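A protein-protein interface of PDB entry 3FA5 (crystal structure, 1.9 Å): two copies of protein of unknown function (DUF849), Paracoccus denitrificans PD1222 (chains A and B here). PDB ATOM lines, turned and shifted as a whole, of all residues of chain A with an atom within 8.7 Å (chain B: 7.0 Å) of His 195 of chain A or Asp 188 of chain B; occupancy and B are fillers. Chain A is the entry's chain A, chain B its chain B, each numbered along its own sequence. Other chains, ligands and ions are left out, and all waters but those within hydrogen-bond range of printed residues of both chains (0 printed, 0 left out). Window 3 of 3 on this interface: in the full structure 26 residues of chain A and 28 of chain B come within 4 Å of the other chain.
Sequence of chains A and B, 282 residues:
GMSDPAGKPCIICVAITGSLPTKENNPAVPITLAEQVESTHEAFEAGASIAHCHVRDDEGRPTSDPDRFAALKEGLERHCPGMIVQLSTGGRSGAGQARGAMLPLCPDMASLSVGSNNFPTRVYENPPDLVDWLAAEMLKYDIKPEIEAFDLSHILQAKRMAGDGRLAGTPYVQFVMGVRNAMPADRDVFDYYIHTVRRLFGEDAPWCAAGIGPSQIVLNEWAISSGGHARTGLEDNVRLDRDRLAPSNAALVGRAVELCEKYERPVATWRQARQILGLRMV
The side-chain carboxylate of Asp 188 of chain A lies within hydrogen-bond range of the side-chain hydroxyl of Tyr 192 of chain B (2.4 Å). The backbone NH (N) of Val 189 of chain A lies close to the side-chain hydroxyl (OH) of Tyr 192 of chain B. The side-chain hydroxyl (OH) of Tyr 192 of chain A sits at hydrogen-bond distance from the backbone carbonyl oxygen (O) of Asp 188 of chain B (3.2 Å). The guanidinium group (NE) of Arg 199 of chain A lies within salt-bridge range of the side-chain carboxylate (OD2) of Asp 188 of chain B. The side-chain hydroxyl (OH) of Tyr 192 of chain A sits close to the backbone NH (N) of Val 189 of chain B. The side-chain carboxylate (OD2) of Asp 186 of chain B lies within salt-bridge range of the guanidinium group (NH2) of Arg 199 of chain A (3.4 Å). A ring nitrogen (NE2) of His 195 of chain A lies within hydrogen-bond range of the side-chain carboxylate (OD2) of Asp 188 of chain B, at 2.9 Å.
N of Val 189 of chain B sits at hydrogen-bond distance from OD1 of Asp 186 of chain B (2.9 Å). N of Asp 188 of chain B sits at hydrogen-bond distance from OD1 of Asp 186 of chain B, at 2.9 Å. O of Tyr 192 of chain A is in hydrogen-bond range of OG1 of Thr 196 of chain A (2.7 Å).
Leu 152 of chain A touches Val 189 of chain B (CD2 to CG1, 3.7 Å). Leu 156 of chain A touches Asp 186 of chain B. Leu 156 of chain A touches Val 189 of chain B. CD1 of Tyr 192 of chain A touches CD1 of Tyr 192 of chain B, at 3.3 Å.
Printed residues of chain B within 4 Å of Asp 188 of chain A: Tyr 192. Phe 190 of chain A touches none of the printed residues of chain B. His 195 of chain A touches one residue of chain B. Of the printed residues of chain B, Arg 199 of chain A touches Asp 186 and Asp 188. Trp 207 of chain A touches none of the printed residues of chain B. The nearest printed residue of chain B that does not touch His 195 of chain A is Val 189 of chain B (7.0 Å). The nearest residue of chain A that does not touch Asp 188 of chain B is Thr 196 of chain A (5.4 Å).
Of the 21 printed residues of chain A, 7 touch a printed residue of chain B. Printed residues of chain A that touch a printed residue of chain B: Leu 152, Leu 156, Asp 188, Val 189, Tyr 192, His 195 and Arg 199. Hydrophobic or aromatic side chains of chain B that line the printed part of chain A: Val 189 and Tyr 192. Among the printed residues, 11 pairs touch across the chains. Among the printed residues, Asp or Glu carboxylates within 4 Å of a Lys or Arg side-chain nitrogen of the other chain: Arg 199 of chain A with Asp 186 of chain B and Arg 199 of chain A with Asp 188 of chain B.
Asp 188 of chain A touches Tyr 192 of chain B, and with the chains exchanged Tyr 192 of chain A touches Asp 188 of chain B. Val 189 of chain A touches Tyr 192 of chain B, and with the chains exchanged Tyr 192 of chain A touches Val 189 of chain B. Tyr 192 of chain A touches its own counterpart, Tyr 192 of chain B. Of the 11 pairs that touch across the chains among the printed residues, 5 have their exchanged pair printed and touching as well.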
ATOM      1  N   LEU A 152      15.490   4.046  -6.263  1.00  0.00           N
ATOM      2  CA  LEU A 152      14.628   5.003  -6.968  1.00  0.00           C
ATOM      3  C   LEU A 152      13.846   4.433  -8.160  1.00  0.00           C
ATOM      4  O   LEU A 152      12.645   4.675  -8.269  1.00  0.00           O
ATOM      5  CB  LEU A 152      15.392   6.231  -7.427  1.00  0.00           C
ATOM      6  CG  LEU A 152      14.562   7.339  -8.085  1.00  0.00           C
ATOM      7  CD1 LEU A 152      13.423   7.856  -7.126  1.00  0.00           C
ATOM      8  CD2 LEU A 152      15.440   8.458  -8.571  1.00  0.00           C
ATOM      9  N   ILE A 155      10.412   2.657  -7.838  1.00  0.00           N
ATOM     10  CA  ILE A 155       9.203   3.491  -7.651  1.00  0.00           C
ATOM     11  C   ILE A 155       8.648   3.846  -9.026  1.00  0.00           C
ATOM     12  O   ILE A 155       7.444   3.607  -9.313  1.00  0.00           O
ATOM     13  CB  ILE A 155       9.473   4.764  -6.788  1.00  0.00           C
ATOM     14  CG1 ILE A 155      10.166   4.383  -5.459  1.00  0.00           C
ATOM     15  CG2 ILE A 155       8.138   5.540  -6.522  1.00  0.00           C
ATOM     16  CD1 ILE A 155      10.536   5.644  -4.550  1.00  0.00           C
ATOM     17  N   LEU A 156       9.546   4.297  -9.915  1.00  0.00           N
ATOM     18  CA  LEU A 156       9.157   4.589 -11.273  1.00  0.00           C
ATOM     19  C   LEU A 156       8.599   3.309 -11.973  1.00  0.00           C
ATOM     20  O   LEU A 156       7.648   3.414 -12.734  1.00  0.00           O
ATOM     21  CB  LEU A 156      10.276   5.290 -12.060  1.00  0.00           C
ATOM     22  CG  LEU A 156      10.442   6.802 -11.893  1.00  0.00           C
ATOM     23  CD1 LEU A 156      10.807   7.109 -10.469  1.00  0.00           C
ATOM     24  CD2 LEU A 156      11.513   7.359 -12.845  1.00  0.00           C
ATOM     25  N   PHE A 175       9.566   2.716   1.271  1.00  0.00           N
ATOM     26  CA  PHE A 175      10.944   3.077   1.123  1.00  0.00           C
ATOM     27  C   PHE A 175      11.805   2.217   2.076  1.00  0.00           C
ATOM     28  O   PHE A 175      11.672   2.329   3.308  1.00  0.00           O
ATOM     29  CB  PHE A 175      11.124   4.578   1.404  1.00  0.00           C
ATOM     30  CG  PHE A 175      10.124   5.446   0.689  1.00  0.00           C
ATOM     31  CD1 PHE A 175       9.632   5.081  -0.581  1.00  0.00           C
ATOM     32  CD2 PHE A 175       9.648   6.600   1.284  1.00  0.00           C
ATOM     33  CE1 PHE A 175       8.675   5.870  -1.239  1.00  0.00           C
ATOM     34  CE2 PHE A 175       8.706   7.407   0.642  1.00  0.00           C
ATOM     35  CZ  PHE A 175       8.203   7.050  -0.604  1.00  0.00           C
ATOM     36  N   ASP A 188      18.104  13.510   2.277  1.00  0.00           N
ATOM     37  CA  ASP A 188      17.891  14.095   0.959  1.00  0.00           C
ATOM     38  C   ASP A 188      17.110  13.136   0.088  1.00  0.00           C
ATOM     39  O   ASP A 188      16.098  13.536  -0.488  1.00  0.00           O
ATOM     40  CB  ASP A 188      19.204  14.519   0.310  1.00  0.00           C
ATOM     41  CG  ASP A 188      19.011  15.474  -0.882  1.00  0.00           C
ATOM     42  OD1 ASP A 188      18.464  15.067  -1.946  1.00  0.00           O
ATOM     43  OD2 ASP A 188      19.471  16.637  -0.769  1.00  0.00           O
ATOM     44  N   VAL A 189      17.562  11.876   0.012  1.00  0.00           N
ATOM     45  CA  VAL A 189      16.942  10.851  -0.844  1.00  0.00           C
ATOM     46  C   VAL A 189      15.522  10.524  -0.370  1.00  0.00           C
ATOM     47  O   VAL A 189      14.608  10.390  -1.192  1.00  0.00           O
ATOM     48  CB  VAL A 189      17.773   9.559  -0.869  1.00  0.00           C
ATOM     49  CG1 VAL A 189      17.056   8.421  -1.653  1.00  0.00           C
ATOM     50  CG2 VAL A 189      19.185   9.842  -1.457  1.00  0.00           C
ATOM     51  N   PHE A 190      15.353  10.438   0.956  1.00  0.00           N
ATOM     52  CA  PHE A 190      14.075  10.109   1.557  1.00  0.00           C
ATOM     53  C   PHE A 190      13.020  11.137   1.107  1.00  0.00           C
ATOM     54  O   PHE A 190      11.916  10.778   0.652  1.00  0.00           O
ATOM     55  CB  PHE A 190      14.200  10.038   3.098  1.00  0.00           C
ATOM     56  CG  PHE A 190      12.869   9.864   3.814  1.00  0.00           C
ATOM     57  CD1 PHE A 190      12.293   8.622   3.967  1.00  0.00           C
ATOM     58  CD2 PHE A 190      12.203  10.955   4.312  1.00  0.00           C
ATOM     59  CE1 PHE A 190      11.071   8.476   4.589  1.00  0.00           C
ATOM     60  CE2 PHE A 190      10.973  10.816   4.971  1.00  0.00           C
ATOM     61  CZ  PHE A 190      10.409   9.584   5.104  1.00  0.00           C
ATOM     62  N   ASP A 191      13.395  12.409   1.196  1.00  0.00           N
ATOM     63  CA  ASP A 191      12.505  13.480   0.786  1.00  0.00           C
ATOM     64  C   ASP A 191      12.189  13.479  -0.706  1.00  0.00           C
ATOM     65  O   ASP A 191      11.043  13.799  -1.078  1.00  0.00           O
ATOM     66  CB  ASP A 191      13.032  14.833   1.271  1.00  0.00           C
ATOM     67  CG  ASP A 191      12.880  14.994   2.776  1.00  0.00           C
ATOM     68  OD1 ASP A 191      12.002  14.323   3.354  1.00  0.00           O
ATOM     69  OD2 ASP A 191      13.599  15.811   3.382  1.00  0.00           O
ATOM     70  N   TYR A 192      13.153  13.040  -1.532  1.00  0.00           N
ATOM     71  CA  TYR A 192      12.954  12.895  -2.974  1.00  0.00           C
ATOM     72  C   TYR A 192      12.031  11.704  -3.253  1.00  0.00           C
ATOM     73  O   TYR A 192      11.217  11.731  -4.166  1.00  0.00           O
ATOM     74  CB  TYR A 192      14.300  12.690  -3.722  1.00  0.00           C
ATOM     75  CG  TYR A 192      14.126  12.772  -5.225  1.00  0.00           C
ATOM     76  CD1 TYR A 192      13.924  14.006  -5.836  1.00  0.00           C
ATOM     77  CD2 TYR A 192      14.123  11.638  -6.026  1.00  0.00           C
ATOM     78  CE1 TYR A 192      13.731  14.118  -7.232  1.00  0.00           C
ATOM     79  CE2 TYR A 192      13.922  11.733  -7.399  1.00  0.00           C
ATOM     80  CZ  TYR A 192      13.729  12.959  -7.990  1.00  0.00           C
ATOM     81  OH  TYR A 192      13.543  13.045  -9.323  1.00  0.00           O
ATOM     82  N   TYR A 193      12.143  10.671  -2.453  1.00  0.00           N
ATOM     83  CA  TYR A 193      11.214   9.565  -2.546  1.00  0.00           C
ATOM     84  C   TYR A 193       9.752  10.046  -2.296  1.00  0.00           C
ATOM     85  O   TYR A 193       8.835   9.646  -2.996  1.00  0.00           O
ATOM     86  CB  TYR A 193      11.589   8.493  -1.533  1.00  0.00           C
ATOM     87  CG  TYR A 193      12.678   7.524  -1.913  1.00  0.00           C
ATOM     88  CD1 TYR A 193      13.274   7.499  -3.179  1.00  0.00           C
ATOM     89  CD2 TYR A 193      13.045   6.564  -1.005  1.00  0.00           C
ATOM     90  CE1 TYR A 193      14.243   6.494  -3.496  1.00  0.00           C
ATOM     91  CE2 TYR A 193      13.982   5.609  -1.271  1.00  0.00           C
ATOM     92  CZ  TYR A 193      14.586   5.552  -2.525  1.00  0.00           C
ATOM     93  OH  TYR A 193      15.523   4.562  -2.720  1.00  0.00           O
ATOM     94  N   ILE A 194       9.556  10.918  -1.309  1.00  0.00           N
ATOM     95  CA  ILE A 194       8.237  11.523  -1.055  1.00  0.00           C
ATOM     96  C   ILE A 194       7.835  12.386  -2.271  1.00  0.00           C
ATOM     97  O   ILE A 194       6.817  12.142  -2.882  1.00  0.00           O
ATOM     98  CB  ILE A 194       8.209  12.354   0.279  1.00  0.00           C
ATOM     99  CG1 ILE A 194       8.406  11.445   1.486  1.00  0.00           C
ATOM    100  CG2 ILE A 194       6.899  13.160   0.378  1.00  0.00           C
ATOM    101  CD1 ILE A 194       8.540  12.159   2.830  1.00  0.00           C
ATOM    102  N   HIS A 195       8.660  13.369  -2.660  1.00  0.00           N
ATOM    103  CA  HIS A 195       8.404  14.104  -3.919  1.00  0.00           C
ATOM    104  C   HIS A 195       7.992  13.170  -5.049  1.00  0.00           C
ATOM    105  O   HIS A 195       7.005  13.421  -5.752  1.00  0.00           O
ATOM    106  CB  HIS A 195       9.630  14.921  -4.328  1.00  0.00           C
ATOM    107  CG  HIS A 195       9.583  15.417  -5.731  1.00  0.00           C
ATOM    108  ND1 HIS A 195       8.871  16.541  -6.105  1.00  0.00           N
ATOM    109  CD2 HIS A 195      10.159  14.938  -6.859  1.00  0.00           C
ATOM    110  CE1 HIS A 195       9.010  16.726  -7.404  1.00  0.00           C
ATOM    111  NE2 HIS A 195       9.775  15.758  -7.889  1.00  0.00           N
ATOM    112  N   THR A 196       8.717  12.071  -5.193  1.00  0.00           N
ATOM    113  CA  THR A 196       8.441  11.106  -6.259  1.00  0.00           C
ATOM    114  C   THR A 196       7.043  10.398  -6.151  1.00  0.00           C
ATOM    115  O   THR A 196       6.271  10.390  -7.110  1.00  0.00           O
ATOM    116  CB  THR A 196       9.640  10.110  -6.438  1.00  0.00           C
ATOM    117  OG1 THR A 196      10.845  10.859  -6.717  1.00  0.00           O
ATOM    118  CG2 THR A 196       9.382   9.183  -7.578  1.00  0.00           C
ATOM    119  N   VAL A 197       6.708   9.827  -5.004  1.00  0.00           N
ATOM    120  CA  VAL A 197       5.392   9.213  -4.831  1.00  0.00           C
ATOM    121  C   VAL A 197       4.282  10.246  -5.077  1.00  0.00           C
ATOM    122  O   VAL A 197       3.271   9.940  -5.722  1.00  0.00           O
ATOM    123  CB  VAL A 197       5.268   8.545  -3.415  1.00  0.00           C
ATOM    124  CG1 VAL A 197       3.832   8.365  -3.009  1.00  0.00           C
ATOM    125  CG2 VAL A 197       6.026   7.226  -3.374  1.00  0.00           C
ATOM    126  N   ARG A 198       4.474  11.470  -4.581  1.00  0.00           N
ATOM    127  CA  ARG A 198       3.448  12.476  -4.689  1.00  0.00           C
ATOM    128  C   ARG A 198       3.174  12.864  -6.129  1.00  0.00           C
ATOM    129  O   ARG A 198       2.027  12.913  -6.517  1.00  0.00           O
ATOM    130  CB  ARG A 198       3.802  13.721  -3.881  1.00  0.00           C
ATOM    131  CG  ARG A 198       3.555  13.529  -2.420  1.00  0.00           C
ATOM    132  CD  ARG A 198       4.140  14.703  -1.588  1.00  0.00           C
ATOM    133  NE  ARG A 198       3.876  14.462  -0.180  1.00  0.00           N
ATOM    134  CZ  ARG A 198       4.317  15.207   0.825  1.00  0.00           C
ATOM    135  NH1 ARG A 198       5.065  16.288   0.603  1.00  0.00           N
ATOM    136  NH2 ARG A 198       3.984  14.871   2.061  1.00  0.00           N
ATOM    137  N   ARG A 199       4.238  13.072  -6.906  1.00  0.00           N
ATOM    138  CA  ARG A 199       4.146  13.474  -8.302  1.00  0.00           C
ATOM    139  C   ARG A 199       3.630  12.345  -9.181  1.00  0.00           C
ATOM    140  O   ARG A 199       2.869  12.603 -10.076  1.00  0.00           O
ATOM    141  CB  ARG A 199       5.492  14.004  -8.844  1.00  0.00           C
ATOM    142  CG  ARG A 199       6.632  12.974  -8.834  1.00  0.00           C
ATOM    143  CD  ARG A 199       7.963  13.531  -9.377  1.00  0.00           C
ATOM    144  NE  ARG A 199       7.908  13.464 -10.819  1.00  0.00           N
ATOM    145  CZ  ARG A 199       8.595  12.647 -11.601  1.00  0.00           C
ATOM    146  NH1 ARG A 199       9.517  11.803 -11.148  1.00  0.00           N
ATOM    147  NH2 ARG A 199       8.351  12.694 -12.893  1.00  0.00           N
ATOM    148  N   LEU A 200       3.997  11.105  -8.905  1.00  0.00           N
ATOM    149  CA  LEU A 200       3.625   9.999  -9.754  1.00  0.00           C
ATOM    150  C   LEU A 200       2.280   9.394  -9.401  1.00  0.00           C
ATOM    151  O   LEU A 200       1.619   8.822 -10.256  1.00  0.00           O
ATOM    152  CB  LEU A 200       4.698   8.890  -9.677  1.00  0.00           C
ATOM    153  CG  LEU A 200       6.062   9.227 -10.299  1.00  0.00           C
ATOM    154  CD1 LEU A 200       6.995   8.068 -10.089  1.00  0.00           C
ATOM    155  CD2 LEU A 200       5.937   9.601 -11.780  1.00  0.00           C
ATOM    156  N   PHE A 201       1.932   9.446  -8.114  1.00  0.00           N
ATOM    157  CA  PHE A 201       0.772   8.750  -7.580  1.00  0.00           C
ATOM    158  C   PHE A 201      -0.286   9.668  -6.949  1.00  0.00           C
ATOM    159  O   PHE A 201      -1.434   9.272  -6.812  1.00  0.00           O
ATOM    160  CB  PHE A 201       1.242   7.740  -6.544  1.00  0.00           C
ATOM    161  CG  PHE A 201       2.133   6.677  -7.103  1.00  0.00           C
ATOM    162  CD1 PHE A 201       1.697   5.870  -8.124  1.00  0.00           C
ATOM    163  CD2 PHE A 201       3.392   6.450  -6.564  1.00  0.00           C
ATOM    164  CE1 PHE A 201       2.541   4.886  -8.666  1.00  0.00           C
ATOM    165  CE2 PHE A 201       4.226   5.462  -7.077  1.00  0.00           C
ATOM    166  CZ  PHE A 201       3.791   4.676  -8.138  1.00  0.00           C
ATOM    167  N   GLY A 202       0.077  10.883  -6.572  1.00  0.00           N
ATOM    168  CA  GLY A 202      -0.897  11.842  -6.039  1.00  0.00           C
ATOM    169  C   GLY A 202      -0.481  12.357  -4.678  1.00  0.00           C
ATOM    170  O   GLY A 202       0.140  11.637  -3.904  1.00  0.00           O
ATOM    171  N   GLU A 203      -0.810  13.617  -4.393  1.00  0.00           N
ATOM    172  CA  GLU A 203      -0.417  14.244  -3.139  1.00  0.00           C
ATOM    173  C   GLU A 203      -0.898  13.473  -1.892  1.00  0.00           C
ATOM    174  O   GLU A 203      -0.312  13.609  -0.841  1.00  0.00           O
ATOM    175  CB  GLU A 203      -0.901  15.685  -3.084  1.00  0.00           C
ATOM    176  CG  GLU A 203      -0.260  16.575  -4.140  1.00  0.00           C
ATOM    177  CD  GLU A 203       1.246  16.802  -3.916  1.00  0.00           C
ATOM    178  OE1 GLU A 203       1.667  17.015  -2.747  1.00  0.00           O
ATOM    179  OE2 GLU A 203       1.987  16.777  -4.925  1.00  0.00           O
ATOM    180  N   TRP A 207       2.026   5.893   1.592  1.00  0.00           N
ATOM    181  CA  TRP A 207       3.340   5.250   1.448  1.00  0.00           C
ATOM    182  C   TRP A 207       3.850   4.933   2.854  1.00  0.00           C
ATOM    183  O   TRP A 207       3.293   5.387   3.847  1.00  0.00           O
ATOM    184  CB  TRP A 207       4.372   6.150   0.712  1.00  0.00           C
ATOM    185  CG  TRP A 207       4.461   7.561   1.253  1.00  0.00           C
ATOM    186  CD1 TRP A 207       3.708   8.622   0.874  1.00  0.00           C
ATOM    187  CD2 TRP A 207       5.338   8.044   2.294  1.00  0.00           C
ATOM    188  NE1 TRP A 207       4.062   9.749   1.613  1.00  0.00           N
ATOM    189  CE2 TRP A 207       5.050   9.415   2.492  1.00  0.00           C
ATOM    190  CE3 TRP A 207       6.321   7.452   3.076  1.00  0.00           C
ATOM    191  CZ2 TRP A 207       5.728  10.208   3.443  1.00  0.00           C
ATOM    192  CZ3 TRP A 207       7.009   8.244   4.019  1.00  0.00           C
ATOM    193  CH2 TRP A 207       6.698   9.610   4.188  1.00  0.00           C
ATOM    194  N   MET B 177      20.262   5.963 -18.662  1.00  0.00           N
ATOM    195  CA  MET B 177      18.800   6.081 -18.726  1.00  0.00           C
ATOM    196  C   MET B 177      18.188   5.496 -19.978  1.00  0.00           C
ATOM    197  O   MET B 177      18.854   5.339 -21.012  1.00  0.00           O
ATOM    198  CB  MET B 177      18.399   7.518 -18.561  1.00  0.00           C
ATOM    199  CG  MET B 177      18.617   7.975 -17.163  1.00  0.00           C
ATOM    200  SD  MET B 177      18.170   9.828 -16.942  1.00  0.00           S
ATOM    201  CE  MET B 177      17.174   9.531 -15.305  1.00  0.00           C
ATOM    202  N   ALA B 185      14.250   7.521 -19.067  1.00  0.00           N
ATOM    203  CA  ALA B 185      14.767   8.868 -19.312  1.00  0.00           C
ATOM    204  C   ALA B 185      13.777   9.905 -18.758  1.00  0.00           C
ATOM    205  O   ALA B 185      12.882  10.347 -19.452  1.00  0.00           O
ATOM    206  CB  ALA B 185      14.981   9.082 -20.834  1.00  0.00           C
ATOM    207  N   ASP B 186      13.981  10.318 -17.513  1.00  0.00           N
ATOM    208  CA  ASP B 186      13.026  11.148 -16.781  1.00  0.00           C
ATOM    209  C   ASP B 186      13.789  12.376 -16.375  1.00  0.00           C
ATOM    210  O   ASP B 186      14.810  12.272 -15.710  1.00  0.00           O
ATOM    211  CB  ASP B 186      12.573  10.375 -15.532  1.00  0.00           C
ATOM    212  CG  ASP B 186      11.595  11.139 -14.666  1.00  0.00           C
ATOM    213  OD1 ASP B 186      11.916  12.185 -14.045  1.00  0.00           O
ATOM    214  OD2 ASP B 186      10.508  10.621 -14.536  1.00  0.00           O
ATOM    215  N   ARG B 187      13.294  13.540 -16.770  1.00  0.00           N
ATOM    216  CA  ARG B 187      14.039  14.784 -16.548  1.00  0.00           C
ATOM    217  C   ARG B 187      14.124  15.126 -15.080  1.00  0.00           C
ATOM    218  O   ARG B 187      15.132  15.693 -14.617  1.00  0.00           O
ATOM    219  CB  ARG B 187      13.409  15.961 -17.280  1.00  0.00           C
ATOM    220  CG  ARG B 187      14.217  17.303 -17.183  1.00  0.00           C
ATOM    221  CD  ARG B 187      15.645  17.044 -17.693  1.00  0.00           C
ATOM    222  NE  ARG B 187      16.537  18.175 -17.472  1.00  0.00           N
ATOM    223  CZ  ARG B 187      16.732  19.144 -18.345  1.00  0.00           C
ATOM    224  NH1 ARG B 187      16.075  19.185 -19.493  1.00  0.00           N
ATOM    225  NH2 ARG B 187      17.568  20.103 -18.041  1.00  0.00           N
ATOM    226  N   ASP B 188      13.056  14.814 -14.342  1.00  0.00           N
ATOM    227  CA  ASP B 188      13.057  15.096 -12.913  1.00  0.00           C
ATOM    228  C   ASP B 188      14.163  14.311 -12.225  1.00  0.00           C
ATOM    229  O   ASP B 188      14.954  14.906 -11.449  1.00  0.00           O
ATOM    230  CB  ASP B 188      11.689  14.812 -12.314  1.00  0.00           C
ATOM    231  CG  ASP B 188      11.534  15.337 -10.891  1.00  0.00           C
ATOM    232  OD1 ASP B 188      12.301  14.933 -10.001  1.00  0.00           O
ATOM    233  OD2 ASP B 188      10.556  16.054 -10.638  1.00  0.00           O
ATOM    234  N   VAL B 189      14.243  13.010 -12.533  1.00  0.00           N
ATOM    235  CA  VAL B 189      15.264  12.126 -11.918  1.00  0.00           C
ATOM    236  C   VAL B 189      16.651  12.598 -12.397  1.00  0.00           C
ATOM    237  O   VAL B 189      17.570  12.760 -11.582  1.00  0.00           O
ATOM    238  CB  VAL B 189      15.008  10.625 -12.225  1.00  0.00           C
ATOM    239  CG1 VAL B 189      16.243   9.750 -11.890  1.00  0.00           C
ATOM    240  CG2 VAL B 189      13.779  10.140 -11.467  1.00  0.00           C
ATOM    241  N   PHE B 190      16.767  12.905 -13.701  1.00  0.00           N
ATOM    242  CA  PHE B 190      18.017  13.430 -14.245  1.00  0.00           C
ATOM    243  C   PHE B 190      18.541  14.623 -13.447  1.00  0.00           C
ATOM    244  O   PHE B 190      19.707  14.618 -13.068  1.00  0.00           O
ATOM    245  CB  PHE B 190      17.881  13.849 -15.708  1.00  0.00           C
ATOM    246  CG  PHE B 190      19.190  14.370 -16.333  1.00  0.00           C
ATOM    247  CD1 PHE B 190      20.122  13.484 -16.845  1.00  0.00           C
ATOM    248  CD2 PHE B 190      19.439  15.738 -16.446  1.00  0.00           C
ATOM    249  CE1 PHE B 190      21.299  13.938 -17.459  1.00  0.00           C
ATOM    250  CE2 PHE B 190      20.597  16.210 -17.047  1.00  0.00           C
ATOM    251  CZ  PHE B 190      21.547  15.300 -17.551  1.00  0.00           C
ATOM    252  N   ASP B 191      17.706  15.634 -13.187  1.00  0.00           N
ATOM    253  CA  ASP B 191      18.196  16.811 -12.429  1.00  0.00           C
ATOM    254  C   ASP B 191      18.570  16.424 -11.000  1.00  0.00           C
ATOM    255  O   ASP B 191      19.439  17.084 -10.373  1.00  0.00           O
ATOM    256  CB  ASP B 191      17.195  17.970 -12.416  1.00  0.00           C
ATOM    257  CG  ASP B 191      16.946  18.533 -13.811  1.00  0.00           C
ATOM    258  OD1 ASP B 191      17.916  18.639 -14.552  1.00  0.00           O
ATOM    259  OD2 ASP B 191      15.803  18.852 -14.163  1.00  0.00           O
ATOM    260  N   TYR B 192      17.916  15.372 -10.499  1.00  0.00           N
ATOM    261  CA  TYR B 192      18.169  14.927  -9.148  1.00  0.00           C
ATOM    262  C   TYR B 192      19.527  14.224  -9.086  1.00  0.00           C
ATOM    263  O   TYR B 192      20.282  14.409  -8.136  1.00  0.00           O
ATOM    264  CB  TYR B 192      17.061  14.022  -8.589  1.00  0.00           C
ATOM    265  CG  TYR B 192      17.300  13.760  -7.110  1.00  0.00           C
ATOM    266  CD1 TYR B 192      17.129  14.752  -6.166  1.00  0.00           C
ATOM    267  CD2 TYR B 192      17.749  12.546  -6.669  1.00  0.00           C
ATOM    268  CE1 TYR B 192      17.364  14.509  -4.828  1.00  0.00           C
ATOM    269  CE2 TYR B 192      17.995  12.297  -5.345  1.00  0.00           C
ATOM    270  CZ  TYR B 192      17.803  13.268  -4.416  1.00  0.00           C
ATOM    271  OH  TYR B 192      18.055  12.981  -3.074  1.00  0.00           O
ATOM    272  N   TYR B 193      19.799  13.406 -10.100  1.00  0.00           N
ATOM    273  CA  TYR B 193      21.123  12.805 -10.286  1.00  0.00           C
ATOM    274  C   TYR B 193      22.241  13.881 -10.287  1.00  0.00           C
ATOM    275  O   TYR B 193      23.268  13.743  -9.631  1.00  0.00           O
ATOM    276  CB  TYR B 193      21.125  12.066 -11.614  1.00  0.00           C
ATOM    277  CG  TYR B 193      20.529  10.679 -11.625  1.00  0.00           C
ATOM    278  CD1 TYR B 193      20.107  10.044 -10.467  1.00  0.00           C
ATOM    279  CD2 TYR B 193      20.560   9.942 -12.795  1.00  0.00           C
ATOM    280  CE1 TYR B 193      19.670   8.700 -10.526  1.00  0.00           C
ATOM    281  CE2 TYR B 193      20.097   8.619 -12.859  1.00  0.00           C
ATOM    282  CZ  TYR B 193      19.662   8.018 -11.736  1.00  0.00           C
ATOM    283  OH  TYR B 193      19.299   6.698 -11.841  1.00  0.00           O
ATOM    284  N   TRP B 222      20.399  16.700 -22.658  1.00  0.00           N
ATOM    285  CA  TRP B 222      20.292  17.007 -21.226  1.00  0.00           C
ATOM    286  C   TRP B 222      21.659  17.238 -20.631  1.00  0.00           C
ATOM    287  O   TRP B 222      21.886  18.263 -19.975  1.00  0.00           O
ATOM    288  CB  TRP B 222      19.538  15.921 -20.437  1.00  0.00           C
ATOM    289  CG  TRP B 222      18.082  15.818 -20.806  1.00  0.00           C
ATOM    290  CD1 TRP B 222      17.377  16.655 -21.626  1.00  0.00           C
ATOM    291  CD2 TRP B 222      17.156  14.845 -20.345  1.00  0.00           C
ATOM    292  NE1 TRP B 222      16.075  16.250 -21.719  1.00  0.00           N
ATOM    293  CE2 TRP B 222      15.909  15.135 -20.947  1.00  0.00           C
ATOM    294  CE3 TRP B 222      17.256  13.745 -19.499  1.00  0.00           C
ATOM    295  CZ2 TRP B 222      14.785  14.355 -20.735  1.00  0.00           C
ATOM    296  CZ3 TRP B 222      16.146  12.988 -19.277  1.00  0.00           C
ATOM    297  CH2 TRP B 222      14.920  13.283 -19.897  1.00  0.00           C
